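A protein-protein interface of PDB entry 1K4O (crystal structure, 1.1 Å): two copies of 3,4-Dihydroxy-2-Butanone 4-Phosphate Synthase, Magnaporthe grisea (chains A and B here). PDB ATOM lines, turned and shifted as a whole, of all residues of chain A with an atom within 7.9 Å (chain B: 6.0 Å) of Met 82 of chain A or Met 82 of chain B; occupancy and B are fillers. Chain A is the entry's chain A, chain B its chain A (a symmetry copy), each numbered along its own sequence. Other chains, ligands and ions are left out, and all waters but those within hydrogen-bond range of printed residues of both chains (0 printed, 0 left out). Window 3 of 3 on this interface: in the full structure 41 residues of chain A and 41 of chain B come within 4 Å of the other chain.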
ATOM      1  N   LEU A  79       4.602 -16.496 -15.676  1.00  0.00           N
ATOM      2  CA  LEU A  79       3.771 -17.636 -16.065  1.00  0.00           C
ATOM      3  C   LEU A  79       2.750 -17.208 -17.094  1.00  0.00           C
ATOM      4  O   LEU A  79       1.623 -16.836 -16.805  1.00  0.00           O
ATOM      5  CB  LEU A  79       3.068 -18.264 -14.829  1.00  0.00           C
ATOM      6  CG  LEU A  79       4.028 -18.721 -13.741  1.00  0.00           C
ATOM      7  CD1 LEU A  79       3.224 -18.966 -12.470  1.00  0.00           C
ATOM      8  CD2 LEU A  79       4.739 -20.007 -14.148  1.00  0.00           C
ATOM      9  N   PRO A  80       3.136 -17.244 -18.360  1.00  0.00           N
ATOM     10  CA  PRO A  80       2.227 -16.826 -19.418  1.00  0.00           C
ATOM     11  C   PRO A  80       1.114 -17.857 -19.640  1.00  0.00           C
ATOM     12  O   PRO A  80       1.239 -19.023 -19.275  1.00  0.00           O
ATOM     13  CB  PRO A  80       3.131 -16.743 -20.662  1.00  0.00           C
ATOM     14  CG  PRO A  80       4.379 -17.573 -20.330  1.00  0.00           C
ATOM     15  CD  PRO A  80       4.511 -17.577 -18.809  1.00  0.00           C
ATOM     16  N   GLN A  81       0.017 -17.450 -20.242  1.00  0.00           N
ATOM     17  CA  GLN A  81      -1.084 -18.349 -20.539  1.00  0.00           C
ATOM     18  C   GLN A  81      -0.631 -19.403 -21.523  1.00  0.00           C
ATOM     19  O   GLN A  81       0.146 -19.145 -22.454  1.00  0.00           O
ATOM     20  CB  GLN A  81      -2.267 -17.589 -21.175  1.00  0.00           C
ATOM     21  CG  GLN A  81      -2.995 -16.702 -20.153  1.00  0.00           C
ATOM     22  CD  GLN A  81      -3.659 -17.538 -19.076  1.00  0.00           C
ATOM     23  OE1 GLN A  81      -3.196 -17.544 -17.905  1.00  0.00           O
ATOM     24  NE2 GLN A  81      -4.727 -18.228 -19.438  1.00  0.00           N
ATOM     25  N   MET A  82      -1.115 -20.623 -21.313  1.00  0.00           N
ATOM     26  CA  MET A  82      -0.765 -21.732 -22.174  1.00  0.00           C
ATOM     27  C   MET A  82      -1.188 -21.436 -23.594  1.00  0.00           C
ATOM     28  O   MET A  82      -0.497 -21.835 -24.542  1.00  0.00           O
ATOM     29  CB  MET A  82      -1.511 -22.986 -21.715  1.00  0.00           C
ATOM     30  CG  MET A  82      -0.921 -24.260 -22.286  1.00  0.00           C
ATOM     31  SD  MET A  82      -1.991 -25.693 -21.857  1.00  0.00           S
ATOM     32  CE  MET A  82      -1.623 -25.858 -20.098  1.00  0.00           C
ATOM     33  N   VAL A  83      -2.343 -20.844 -23.763  1.00  0.00           N
ATOM     34  CA  VAL A  83      -2.757 -20.497 -25.090  1.00  0.00           C
ATOM     35  C   VAL A  83      -3.142 -19.025 -25.162  1.00  0.00           C
ATOM     36  O   VAL A  83      -3.875 -18.527 -24.311  1.00  0.00           O
ATOM     37  CB  VAL A  83      -3.712 -21.475 -25.773  1.00  0.00           C
ATOM     38  CG1 VAL A  83      -3.761 -22.842 -25.117  1.00  0.00           C
ATOM     39  CG2 VAL A  83      -5.100 -20.913 -25.955  1.00  0.00           C
ATOM     40  N   THR A  84      -2.641 -18.348 -26.199  1.00  0.00           N
ATOM     41  CA  THR A  84      -2.908 -16.938 -26.503  1.00  0.00           C
ATOM     42  C   THR A  84      -4.365 -16.636 -26.883  1.00  0.00           C
ATOM     43  O   THR A  84      -4.920 -15.600 -26.487  1.00  0.00           O
ATOM     44  CB  THR A  84      -1.962 -16.554 -27.646  1.00  0.00           C
ATOM     45  OG1 THR A  84      -2.322 -17.315 -28.796  1.00  0.00           O
ATOM     46  CG2 THR A  84      -0.557 -16.934 -27.196  1.00  0.00           C
ATOM     47  N   HIS A  85      -5.021 -17.530 -27.621  1.00  0.00           N
ATOM     48  CA  HIS A  85      -6.425 -17.350 -28.003  1.00  0.00           C
ATOM     49  C   HIS A  85      -7.307 -18.523 -27.544  1.00  0.00           C
ATOM     50  O   HIS A  85      -7.660 -19.421 -28.326  1.00  0.00           O
ATOM     51  CB  HIS A  85      -6.616 -17.127 -29.512  1.00  0.00           C
ATOM     52  CG  HIS A  85      -6.440 -15.691 -29.892  1.00  0.00           C
ATOM     53  ND1 HIS A  85      -7.406 -14.726 -29.586  1.00  0.00           N
ATOM     54  CD2 HIS A  85      -5.398 -15.088 -30.544  1.00  0.00           C
ATOM     55  CE1 HIS A  85      -6.930 -13.567 -30.057  1.00  0.00           C
ATOM     56  NE2 HIS A  85      -5.728 -13.752 -30.635  1.00  0.00           N
ATOM     57  N   ASN A  86      -7.607 -18.507 -26.252  1.00  0.00           N
ATOM     58  CA  ASN A  86      -8.376 -19.539 -25.561  1.00  0.00           C
ATOM     59  C   ASN A  86      -9.640 -20.106 -26.224  1.00  0.00           C
ATOM     60  O   ASN A  86     -10.515 -19.335 -26.665  1.00  0.00           O
ATOM     61  CB  ASN A  86      -8.583 -19.105 -24.102  1.00  0.00           C
ATOM     62  CG  ASN A  86      -8.624 -20.242 -23.097  1.00  0.00           C
ATOM     63  OD1 ASN A  86      -9.520 -21.099 -23.240  1.00  0.00           O
ATOM     64  ND2 ASN A  86      -7.715 -20.222 -22.082  1.00  0.00           N
ATOM     65  N   THR A  92     -11.063 -21.495 -18.401  1.00  0.00           N
ATOM     66  CA  THR A  92     -10.067 -21.691 -17.366  1.00  0.00           C
ATOM     67  C   THR A  92      -8.752 -21.155 -17.933  1.00  0.00           C
ATOM     68  O   THR A  92      -8.308 -21.496 -19.024  1.00  0.00           O
ATOM     69  CB  THR A  92      -9.981 -23.201 -17.076  1.00  0.00           C
ATOM     70  OG1 THR A  92     -11.245 -23.673 -16.615  1.00  0.00           O
ATOM     71  CG2 THR A  92      -8.931 -23.506 -16.031  1.00  0.00           C
ATOM     72  N   ALA A  93      -8.118 -20.293 -17.159  1.00  0.00           N
ATOM     73  CA  ALA A  93      -6.914 -19.606 -17.560  1.00  0.00           C
ATOM     74  C   ALA A  93      -5.636 -20.303 -17.236  1.00  0.00           C
ATOM     75  O   ALA A  93      -4.835 -19.846 -16.432  1.00  0.00           O
ATOM     76  CB  ALA A  93      -6.983 -18.197 -16.997  1.00  0.00           C
ATOM     77  N   TYR A  94      -5.435 -21.455 -17.851  1.00  0.00           N
ATOM     78  CA  TYR A  94      -4.227 -22.175 -17.585  1.00  0.00           C
ATOM     79  C   TYR A  94      -2.969 -21.411 -17.992  1.00  0.00           C
ATOM     80  O   TYR A  94      -2.914 -20.904 -19.131  1.00  0.00           O
ATOM     81  CB  TYR A  94      -4.147 -23.460 -18.459  1.00  0.00           C
ATOM     82  CG  TYR A  94      -5.253 -24.438 -18.163  1.00  0.00           C
ATOM     83  CD1 TYR A  94      -6.394 -24.486 -18.963  1.00  0.00           C
ATOM     84  CD2 TYR A  94      -5.111 -25.291 -17.073  1.00  0.00           C
ATOM     85  CE1 TYR A  94      -7.419 -25.384 -18.665  1.00  0.00           C
ATOM     86  CE2 TYR A  94      -6.133 -26.188 -16.769  1.00  0.00           C
ATOM     87  CZ  TYR A  94      -7.273 -26.218 -17.560  1.00  0.00           C
ATOM     88  OH  TYR A  94      -8.246 -27.118 -17.172  1.00  0.00           O
ATOM     89  N   THR A  95      -1.940 -21.399 -17.136  1.00  0.00           N
ATOM     90  CA  THR A  95      -0.660 -20.843 -17.576  1.00  0.00           C
ATOM     91  C   THR A  95       0.148 -22.044 -18.063  1.00  0.00           C
ATOM     92  O   THR A  95      -0.297 -23.204 -18.018  1.00  0.00           O
ATOM     93  CB  THR A  95       0.163 -20.194 -16.412  1.00  0.00           C
ATOM     94  OG1 THR A  95       0.587 -21.174 -15.461  1.00  0.00           O
ATOM     95  CG2 THR A  95      -0.661 -19.150 -15.654  1.00  0.00           C
ATOM     96  N   VAL A  96       1.405 -21.802 -18.458  1.00  0.00           N
ATOM     97  CA  VAL A  96       2.288 -22.903 -18.771  1.00  0.00           C
ATOM     98  C   VAL A  96       2.411 -23.700 -17.436  1.00  0.00           C
ATOM     99  O   VAL A  96       2.324 -23.147 -16.315  1.00  0.00           O
ATOM    100  CB  VAL A  96       3.650 -22.346 -19.211  1.00  0.00           C
ATOM    101  CG1 VAL A  96       4.283 -21.513 -18.102  1.00  0.00           C
ATOM    102  CG2 VAL A  96       4.604 -23.469 -19.547  1.00  0.00           C
ATOM    103  N   SER A  97       2.569 -25.030 -17.530  1.00  0.00           N
ATOM    104  CA  SER A  97       2.696 -25.903 -16.370  1.00  0.00           C
ATOM    105  C   SER A  97       4.097 -25.823 -15.787  1.00  0.00           C
ATOM    106  O   SER A  97       5.062 -25.427 -16.458  1.00  0.00           O
ATOM    107  CB  SER A  97       2.330 -27.324 -16.756  1.00  0.00           C
ATOM    108  OG  SER A  97       3.138 -27.730 -17.841  1.00  0.00           O
ATOM    109  N   VAL A  98       4.230 -26.250 -14.523  1.00  0.00           N
ATOM    110  CA  VAL A  98       5.505 -26.149 -13.841  1.00  0.00           C
ATOM    111  C   VAL A  98       5.815 -27.340 -12.951  1.00  0.00           C
ATOM    112  O   VAL A  98       4.938 -28.067 -12.481  1.00  0.00           O
ATOM    113  CB  VAL A  98       5.483 -24.926 -12.871  1.00  0.00           C
ATOM    114  CG1 VAL A  98       5.263 -23.609 -13.645  1.00  0.00           C
ATOM    115  CG2 VAL A  98       4.450 -25.020 -11.728  1.00  0.00           C
ATOM    116  N   ARG A 133       9.636 -25.344 -16.630  1.00  0.00           N
ATOM    117  CA  ARG A 133       8.460 -25.362 -17.492  1.00  0.00           C
ATOM    118  C   ARG A 133       8.799 -26.242 -18.699  1.00  0.00           C
ATOM    119  O   ARG A 133       9.895 -26.145 -19.216  1.00  0.00           O
ATOM    120  CB  ARG A 133       8.135 -23.963 -17.993  1.00  0.00           C
ATOM    121  CG  ARG A 133       8.000 -22.919 -16.879  1.00  0.00           C
ATOM    122  CD  ARG A 133       9.327 -22.152 -16.686  1.00  0.00           C
ATOM    123  NE  ARG A 133       9.373 -21.204 -15.534  1.00  0.00           N
ATOM    124  CZ  ARG A 133       8.617 -20.110 -15.486  1.00  0.00           C
ATOM    125  NH1 ARG A 133       7.815 -19.775 -16.513  1.00  0.00           N
ATOM    126  NH2 ARG A 133       8.701 -19.321 -14.401  1.00  0.00           N
ATOM    127  N   PRO A 134       7.905 -27.093 -19.182  1.00  0.00           N
ATOM    128  CA  PRO A 134       6.595 -27.381 -18.651  1.00  0.00           C
ATOM    129  C   PRO A 134       6.804 -28.305 -17.467  1.00  0.00           C
ATOM    130  O   PRO A 134       7.928 -28.651 -17.085  1.00  0.00           O
ATOM    131  CB  PRO A 134       5.889 -28.114 -19.787  1.00  0.00           C
ATOM    132  CG  PRO A 134       7.013 -28.754 -20.590  1.00  0.00           C
ATOM    133  CD  PRO A 134       8.249 -27.874 -20.393  1.00  0.00           C
ATOM    134  N   GLY A 135       5.698 -28.716 -16.867  1.00  0.00           N
ATOM    135  CA  GLY A 135       5.771 -29.564 -15.694  1.00  0.00           C
ATOM    136  C   GLY A 135       4.433 -30.231 -15.402  1.00  0.00           C
ATOM    137  O   GLY A 135       3.614 -30.413 -16.310  1.00  0.00           O
ATOM    138  N   VAL A 137       2.229 -29.382 -12.501  1.00  0.00           N
ATOM    139  CA  VAL A 137       1.280 -28.592 -11.716  1.00  0.00           C
ATOM    140  C   VAL A 137       0.798 -27.495 -12.653  1.00  0.00           C
ATOM    141  O   VAL A 137       1.596 -26.942 -13.426  1.00  0.00           O
ATOM    142  CB  VAL A 137       1.845 -28.070 -10.389  1.00  0.00           C
ATOM    143  CG1 VAL A 137       0.952 -26.979  -9.779  1.00  0.00           C
ATOM    144  CG2 VAL A 137       2.057 -29.241  -9.410  1.00  0.00           C
ATOM    145  N   PHE A 138      -0.472 -27.173 -12.584  1.00  0.00           N
ATOM    146  CA  PHE A 138      -1.126 -26.251 -13.508  1.00  0.00           C
ATOM    147  C   PHE A 138      -1.639 -24.983 -12.865  1.00  0.00           C
ATOM    148  O   PHE A 138      -2.752 -24.931 -12.369  1.00  0.00           O
ATOM    149  CB  PHE A 138      -2.286 -27.022 -14.194  1.00  0.00           C
ATOM    150  CG  PHE A 138      -1.708 -28.176 -14.989  1.00  0.00           C
ATOM    151  CD1 PHE A 138      -1.566 -29.437 -14.418  1.00  0.00           C
ATOM    152  CD2 PHE A 138      -1.299 -28.005 -16.311  1.00  0.00           C
ATOM    153  CE1 PHE A 138      -1.023 -30.482 -15.170  1.00  0.00           C
ATOM    154  CE2 PHE A 138      -0.713 -29.020 -17.067  1.00  0.00           C
ATOM    155  CZ  PHE A 138      -0.569 -30.266 -16.467  1.00  0.00           C
ATOM    156  N   PRO A 139      -0.818 -23.939 -12.890  1.00  0.00           N
ATOM    157  CA  PRO A 139      -1.276 -22.649 -12.322  1.00  0.00           C
ATOM    158  C   PRO A 139      -2.434 -22.095 -13.133  1.00  0.00           C
ATOM    159  O   PRO A 139      -2.479 -22.284 -14.350  1.00  0.00           O
ATOM    160  CB  PRO A 139      -0.056 -21.724 -12.334  1.00  0.00           C
ATOM    161  CG  PRO A 139       1.139 -22.654 -12.517  1.00  0.00           C
ATOM    162  CD  PRO A 139       0.587 -23.851 -13.328  1.00  0.00           C
ATOM    163  N   LEU A 140      -3.387 -21.443 -12.476  1.00  0.00           N
ATOM    164  CA  LEU A 140      -4.555 -20.903 -13.143  1.00  0.00           C
ATOM    165  C   LEU A 140      -4.686 -19.438 -12.747  1.00  0.00           C
ATOM    166  O   LEU A 140      -4.668 -19.118 -11.556  1.00  0.00           O
ATOM    167  CB  LEU A 140      -5.864 -21.583 -12.708  1.00  0.00           C
ATOM    168  CG  LEU A 140      -5.844 -23.103 -12.868  1.00  0.00           C
ATOM    169  CD1 LEU A 140      -7.187 -23.627 -12.363  1.00  0.00           C
ATOM    170  CD2 LEU A 140      -5.626 -23.442 -14.347  1.00  0.00           C
ATOM    171  N   PRO B  80       0.689 -27.907 -31.400  1.00  0.00           N
ATOM    172  CA  PRO B  80       2.037 -27.402 -31.180  1.00  0.00           C
ATOM    173  C   PRO B  80       2.521 -27.697 -29.755  1.00  0.00           C
ATOM    174  O   PRO B  80       1.729 -27.935 -28.846  1.00  0.00           O
ATOM    175  CB  PRO B  80       1.894 -25.883 -31.388  1.00  0.00           C
ATOM    176  CG  PRO B  80       0.396 -25.578 -31.243  1.00  0.00           C
ATOM    177  CD  PRO B  80      -0.349 -26.865 -31.595  1.00  0.00           C
ATOM    178  N   GLN B  81       3.818 -27.682 -29.535  1.00  0.00           N
ATOM    179  CA  GLN B  81       4.385 -27.908 -28.219  1.00  0.00           C
ATOM    180  C   GLN B  81       3.957 -26.803 -27.282  1.00  0.00           C
ATOM    181  O   GLN B  81       3.861 -25.623 -27.653  1.00  0.00           O
ATOM    182  CB  GLN B  81       5.928 -27.911 -28.269  1.00  0.00           C
ATOM    183  CG  GLN B  81       6.477 -29.175 -28.949  1.00  0.00           C
ATOM    184  CD  GLN B  81       6.154 -30.417 -28.142  1.00  0.00           C
ATOM    185  OE1 GLN B  81       5.298 -31.239 -28.562  1.00  0.00           O
ATOM    186  NE2 GLN B  81       6.819 -30.576 -27.010  1.00  0.00           N
ATOM    187  N   MET B  82       3.680 -27.184 -26.039  1.00  0.00           N
ATOM    188  CA  MET B  82       3.255 -26.234 -25.034  1.00  0.00           C
ATOM    189  C   MET B  82       4.319 -25.179 -24.839  1.00  0.00           C
ATOM    190  O   MET B  82       3.994 -24.009 -24.589  1.00  0.00           O
ATOM    191  CB  MET B  82       3.063 -26.957 -23.700  1.00  0.00           C
ATOM    192  CG  MET B  82       2.252 -26.148 -22.707  1.00  0.00           C
ATOM    193  SD  MET B  82       2.242 -26.991 -21.073  1.00  0.00           S
ATOM    194  CE  MET B  82       1.138 -28.374 -21.428  1.00  0.00           C
ATOM    195  N   VAL B  83       5.565 -25.579 -24.845  1.00  0.00           N
ATOM    196  CA  VAL B  83       6.607 -24.603 -24.716  1.00  0.00           C
ATOM    197  C   VAL B  83       7.620 -24.752 -25.844  1.00  0.00           C
ATOM    198  O   VAL B  83       8.065 -25.857 -26.145  1.00  0.00           O
ATOM    199  CB  VAL B  83       7.185 -24.418 -23.314  1.00  0.00           C
ATOM    200  CG1 VAL B  83       6.314 -24.990 -22.212  1.00  0.00           C
ATOM    201  CG2 VAL B  83       8.605 -24.913 -23.193  1.00  0.00           C
ATOM    202  N   THR B  84       7.980 -23.617 -26.451  1.00  0.00           N
ATOM    203  CA  THR B  84       8.969 -23.505 -27.527  1.00  0.00           C
ATOM    204  C   THR B  84      10.406 -23.850 -27.107  1.00  0.00           C
ATOM    205  O   THR B  84      11.151 -24.482 -27.869  1.00  0.00           O
ATOM    206  CB  THR B  84       8.890 -22.062 -28.040  1.00  0.00           C
ATOM    207  OG1 THR B  84       9.301 -21.193 -26.988  1.00  0.00           O
ATOM    208  CG2 THR B  84       7.428 -21.800 -28.382  1.00  0.00           C
ATOM    209  N   TYR B  94       5.208 -32.235 -24.166  1.00  0.00           N
ATOM    210  CA  TYR B  94       3.821 -31.893 -24.090  1.00  0.00           C
ATOM    211  C   TYR B  94       3.365 -30.967 -25.215  1.00  0.00           C
ATOM    212  O   TYR B  94       4.036 -29.945 -25.463  1.00  0.00           O
ATOM    213  CB  TYR B  94       3.530 -31.052 -22.813  1.00  0.00           C
ATOM    214  CG  TYR B  94       3.814 -31.804 -21.540  1.00  0.00           C
ATOM    215  CD1 TYR B  94       5.018 -31.624 -20.861  1.00  0.00           C
ATOM    216  CD2 TYR B  94       2.850 -32.684 -21.058  1.00  0.00           C
ATOM    217  CE1 TYR B  94       5.276 -32.342 -19.692  1.00  0.00           C
ATOM    218  CE2 TYR B  94       3.103 -33.406 -19.894  1.00  0.00           C
ATOM    219  CZ  TYR B  94       4.311 -33.233 -19.233  1.00  0.00           C
ATOM    220  OH  TYR B  94       4.489 -34.007 -18.103  1.00  0.00           O
ATOM    221  N   THR B  95       2.208 -31.248 -25.826  1.00  0.00           N
ATOM    222  CA  THR B  95       1.652 -30.278 -26.771  1.00  0.00           C
ATOM    223  C   THR B  95       0.669 -29.444 -25.950  1.00  0.00           C
ATOM    224  O   THR B  95       0.460 -29.664 -24.744  1.00  0.00           O
ATOM    225  CB  THR B  95       0.822 -30.942 -27.921  1.00  0.00           C
ATOM    226  OG1 THR B  95      -0.363 -31.566 -27.418  1.00  0.00           O
ATOM    227  CG2 THR B  95       1.630 -32.020 -28.648  1.00  0.00           C
ATOM    228  N   VAL B  96      -0.032 -28.517 -26.616  1.00  0.00           N
ATOM    229  CA  VAL B  96      -1.100 -27.805 -25.950  1.00  0.00           C
ATOM    230  C   VAL B  96      -2.127 -28.912 -25.559  1.00  0.00           C
ATOM    231  O   VAL B  96      -2.274 -29.958 -26.232  1.00  0.00           O
ATOM    232  CB  VAL B  96      -1.719 -26.797 -26.929  1.00  0.00           C
ATOM    233  CG1 VAL B  96      -2.293 -27.504 -28.152  1.00  0.00           C
ATOM    234  CG2 VAL B  96      -2.843 -26.030 -26.269  1.00  0.00           C
ATOM    235  N   SER B  97      -2.827 -28.724 -24.428  1.00  0.00           N
ATOM    236  CA  SER B  97      -3.818 -29.672 -23.937  1.00  0.00           C
ATOM    237  C   SER B  97      -5.119 -29.541 -24.711  1.00  0.00           C
ATOM    238  O   SER B  97      -5.406 -28.509 -25.336  1.00  0.00           O
ATOM    239  CB  SER B  97      -4.029 -29.467 -22.448  1.00  0.00           C
ATOM    240  OG  SER B  97      -4.392 -28.122 -22.215  1.00  0.00           O
ATOM    241  N   PRO B 134      -7.251 -24.739 -24.519  1.00  0.00           N
ATOM    242  CA  PRO B 134      -6.585 -25.810 -23.819  1.00  0.00           C
ATOM    243  C   PRO B 134      -7.674 -26.741 -23.321  1.00  0.00           C
ATOM    244  O   PRO B 134      -8.872 -26.550 -23.562  1.00  0.00           O
ATOM    245  CB  PRO B 134      -5.897 -25.115 -22.649  1.00  0.00           C
ATOM    246  CG  PRO B 134      -6.733 -23.867 -22.396  1.00  0.00           C
ATOM    247  CD  PRO B 134      -7.372 -23.489 -23.734  1.00  0.00           C
ATOM    248  N   GLY B 135      -7.255 -27.775 -22.610  1.00  0.00           N
ATOM    249  CA  GLY B 135      -8.198 -28.761 -22.120  1.00  0.00           C
ATOM    250  C   GLY B 135      -7.586 -29.624 -21.024  1.00  0.00           C
ATOM    251  O   GLY B 135      -6.651 -29.195 -20.340  1.00  0.00           O
ATOM    252  N   PHE B 138      -3.528 -34.465 -22.225  1.00  0.00           N
ATOM    253  CA  PHE B 138      -2.203 -33.972 -22.585  1.00  0.00           C
ATOM    254  C   PHE B 138      -1.484 -34.808 -23.620  1.00  0.00           C
ATOM    255  O   PHE B 138      -0.802 -35.765 -23.295  1.00  0.00           O
ATOM    256  CB  PHE B 138      -1.366 -33.884 -21.279  1.00  0.00           C
ATOM    257  CG  PHE B 138      -2.018 -32.885 -20.344  1.00  0.00           C
ATOM    258  CD1 PHE B 138      -2.953 -33.296 -19.399  1.00  0.00           C
ATOM    259  CD2 PHE B 138      -1.702 -31.529 -20.407  1.00  0.00           C
ATOM    260  CE1 PHE B 138      -3.546 -32.353 -18.554  1.00  0.00           C
ATOM    261  CE2 PHE B 138      -2.312 -30.564 -19.606  1.00  0.00           C
ATOM    262  CZ  PHE B 138      -3.254 -30.999 -18.681  1.00  0.00           C
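Hydrophobic or aromatic side chains of chain B that line the printed part of chain A: Met 82, Val 83, Tyr 94, Val 96, Pro 134 and Phe 138.
Among the printed residues, 11 pairs touch across the chains.
Among the printed residues, no Asp or Glu carboxylate lies within 4 Å of a Lys or Arg side-chain nitrogen of the other chain.
Of chain B, only Met 82 and Ser 97 come within 4 Å of Met 82 of chain A.
Of the printed residues of chain B, Val 83 of chain A touches Val 96 and Pro 134.
Pro 139 of chain A touches none of the printed residues of chain B.
Of chain A, only Met 82 (3.7 Å) and Ser 97 (3.4 Å) come within 4 Å of Met 82 of chain B.
Printed residues of chain A within 4 Å of Tyr 94 of chain B: Pro 134 (3.5 Å).
Of the printed residues of chain A, Pro 134 of chain B touches Val 83 (3.9 Å), Asn 86 (3.3 Å) and Tyr 94 (3.5 Å).
The nearest printed residue of chain B that does not touch Phe 138 of chain A is Met 82 of chain B (4.8 Å).
Met 82 of chain A touches Ser 97 of chain B, and with the chains exchanged Ser 97 of chain A touches Met 82 of chain B.
Val 83 of chain A touches Val 96 of chain B, and with the chains exchanged Val 96 of chain A touches Val 83 of chain B.
Val 83 of chain A touches Pro 134 of chain B, and with the chains exchanged Pro 134 of chain A touches Val 83 of chain B.
Tyr 94 of chain A touches Pro 134 of chain B, and with the chains exchanged Pro 134 of chain A touches Tyr 94 of chain B.
Positions printed for both chains: 80, 81, 82, 83, 84, 94, 95, 96, 97, 134, 135 and 138.
Of the 11 pairs that touch across the chains among the printed residues, 10 have their exchanged pair printed and touching as well.
SD of Met 82 of chain A lies within hydrogen-bond range of OG of Ser 97 of chain B (3.4 Å).
The side-chain hydroxyl (OG) of Ser 97 of chain A lies within hydrogen-bond range of the side-chain sulfur (SD) of Met 82 of chain B (3.4 Å).
Among the printed residues, merely in contact across the chains: Asn 86 of chain A with Pro 134 of chain B (3.3 Å), Phe 138 of chain A with Phe 138 of chain B (3.4 Å), Tyr 94 of chain A with Pro 134 of chain B (3.5 Å), Pro 134 of chain A with Tyr 94 of chain B (3.5 Å), Val 83 of chain A with Val 96 of chain B (3.5 Å), Val 96 of chain A with Val 83 of chain B (3.5 Å), Met 82 of chain A with Met 82 of chain B (3.7 Å), Pro 134 of chain A with Val 83 of chain B (3.9 Å) and Val 83 of chain A with Pro 134 of chain B (3.9 Å).
The backbone NH (N) of Val 96 of chain A sits at hydrogen-bond distance from the backbone carbonyl oxygen (O) of Pro 80 of chain A, at 2.9 Å.
NE2 of Gln 81 of chain A lies within hydrogen-bond range of O of Tyr 94 of chain A, 3.2 Å away.
The side-chain hydroxyl (OG) of Ser 97 of chain A sits at hydrogen-bond distance from the backbone NH (N) of Gly 135 of chain A, at 2.9 Å.
N of Val 96 of chain B sits at hydrogen-bond distance from O of Pro 80 of chain B, at 2.9 Å.
The side-chain amide nitrogen (NE2) of Gln 81 of chain B is in hydrogen-bond range of the backbone carbonyl oxygen (O) of Tyr 94 of chain B, at 3.2 Å.
The backbone carbonyl oxygen (O) of Tyr 94 of chain B lies within hydrogen-bond range of the backbone NH (N) of Met 82 of chain B, at 2.8 Å.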
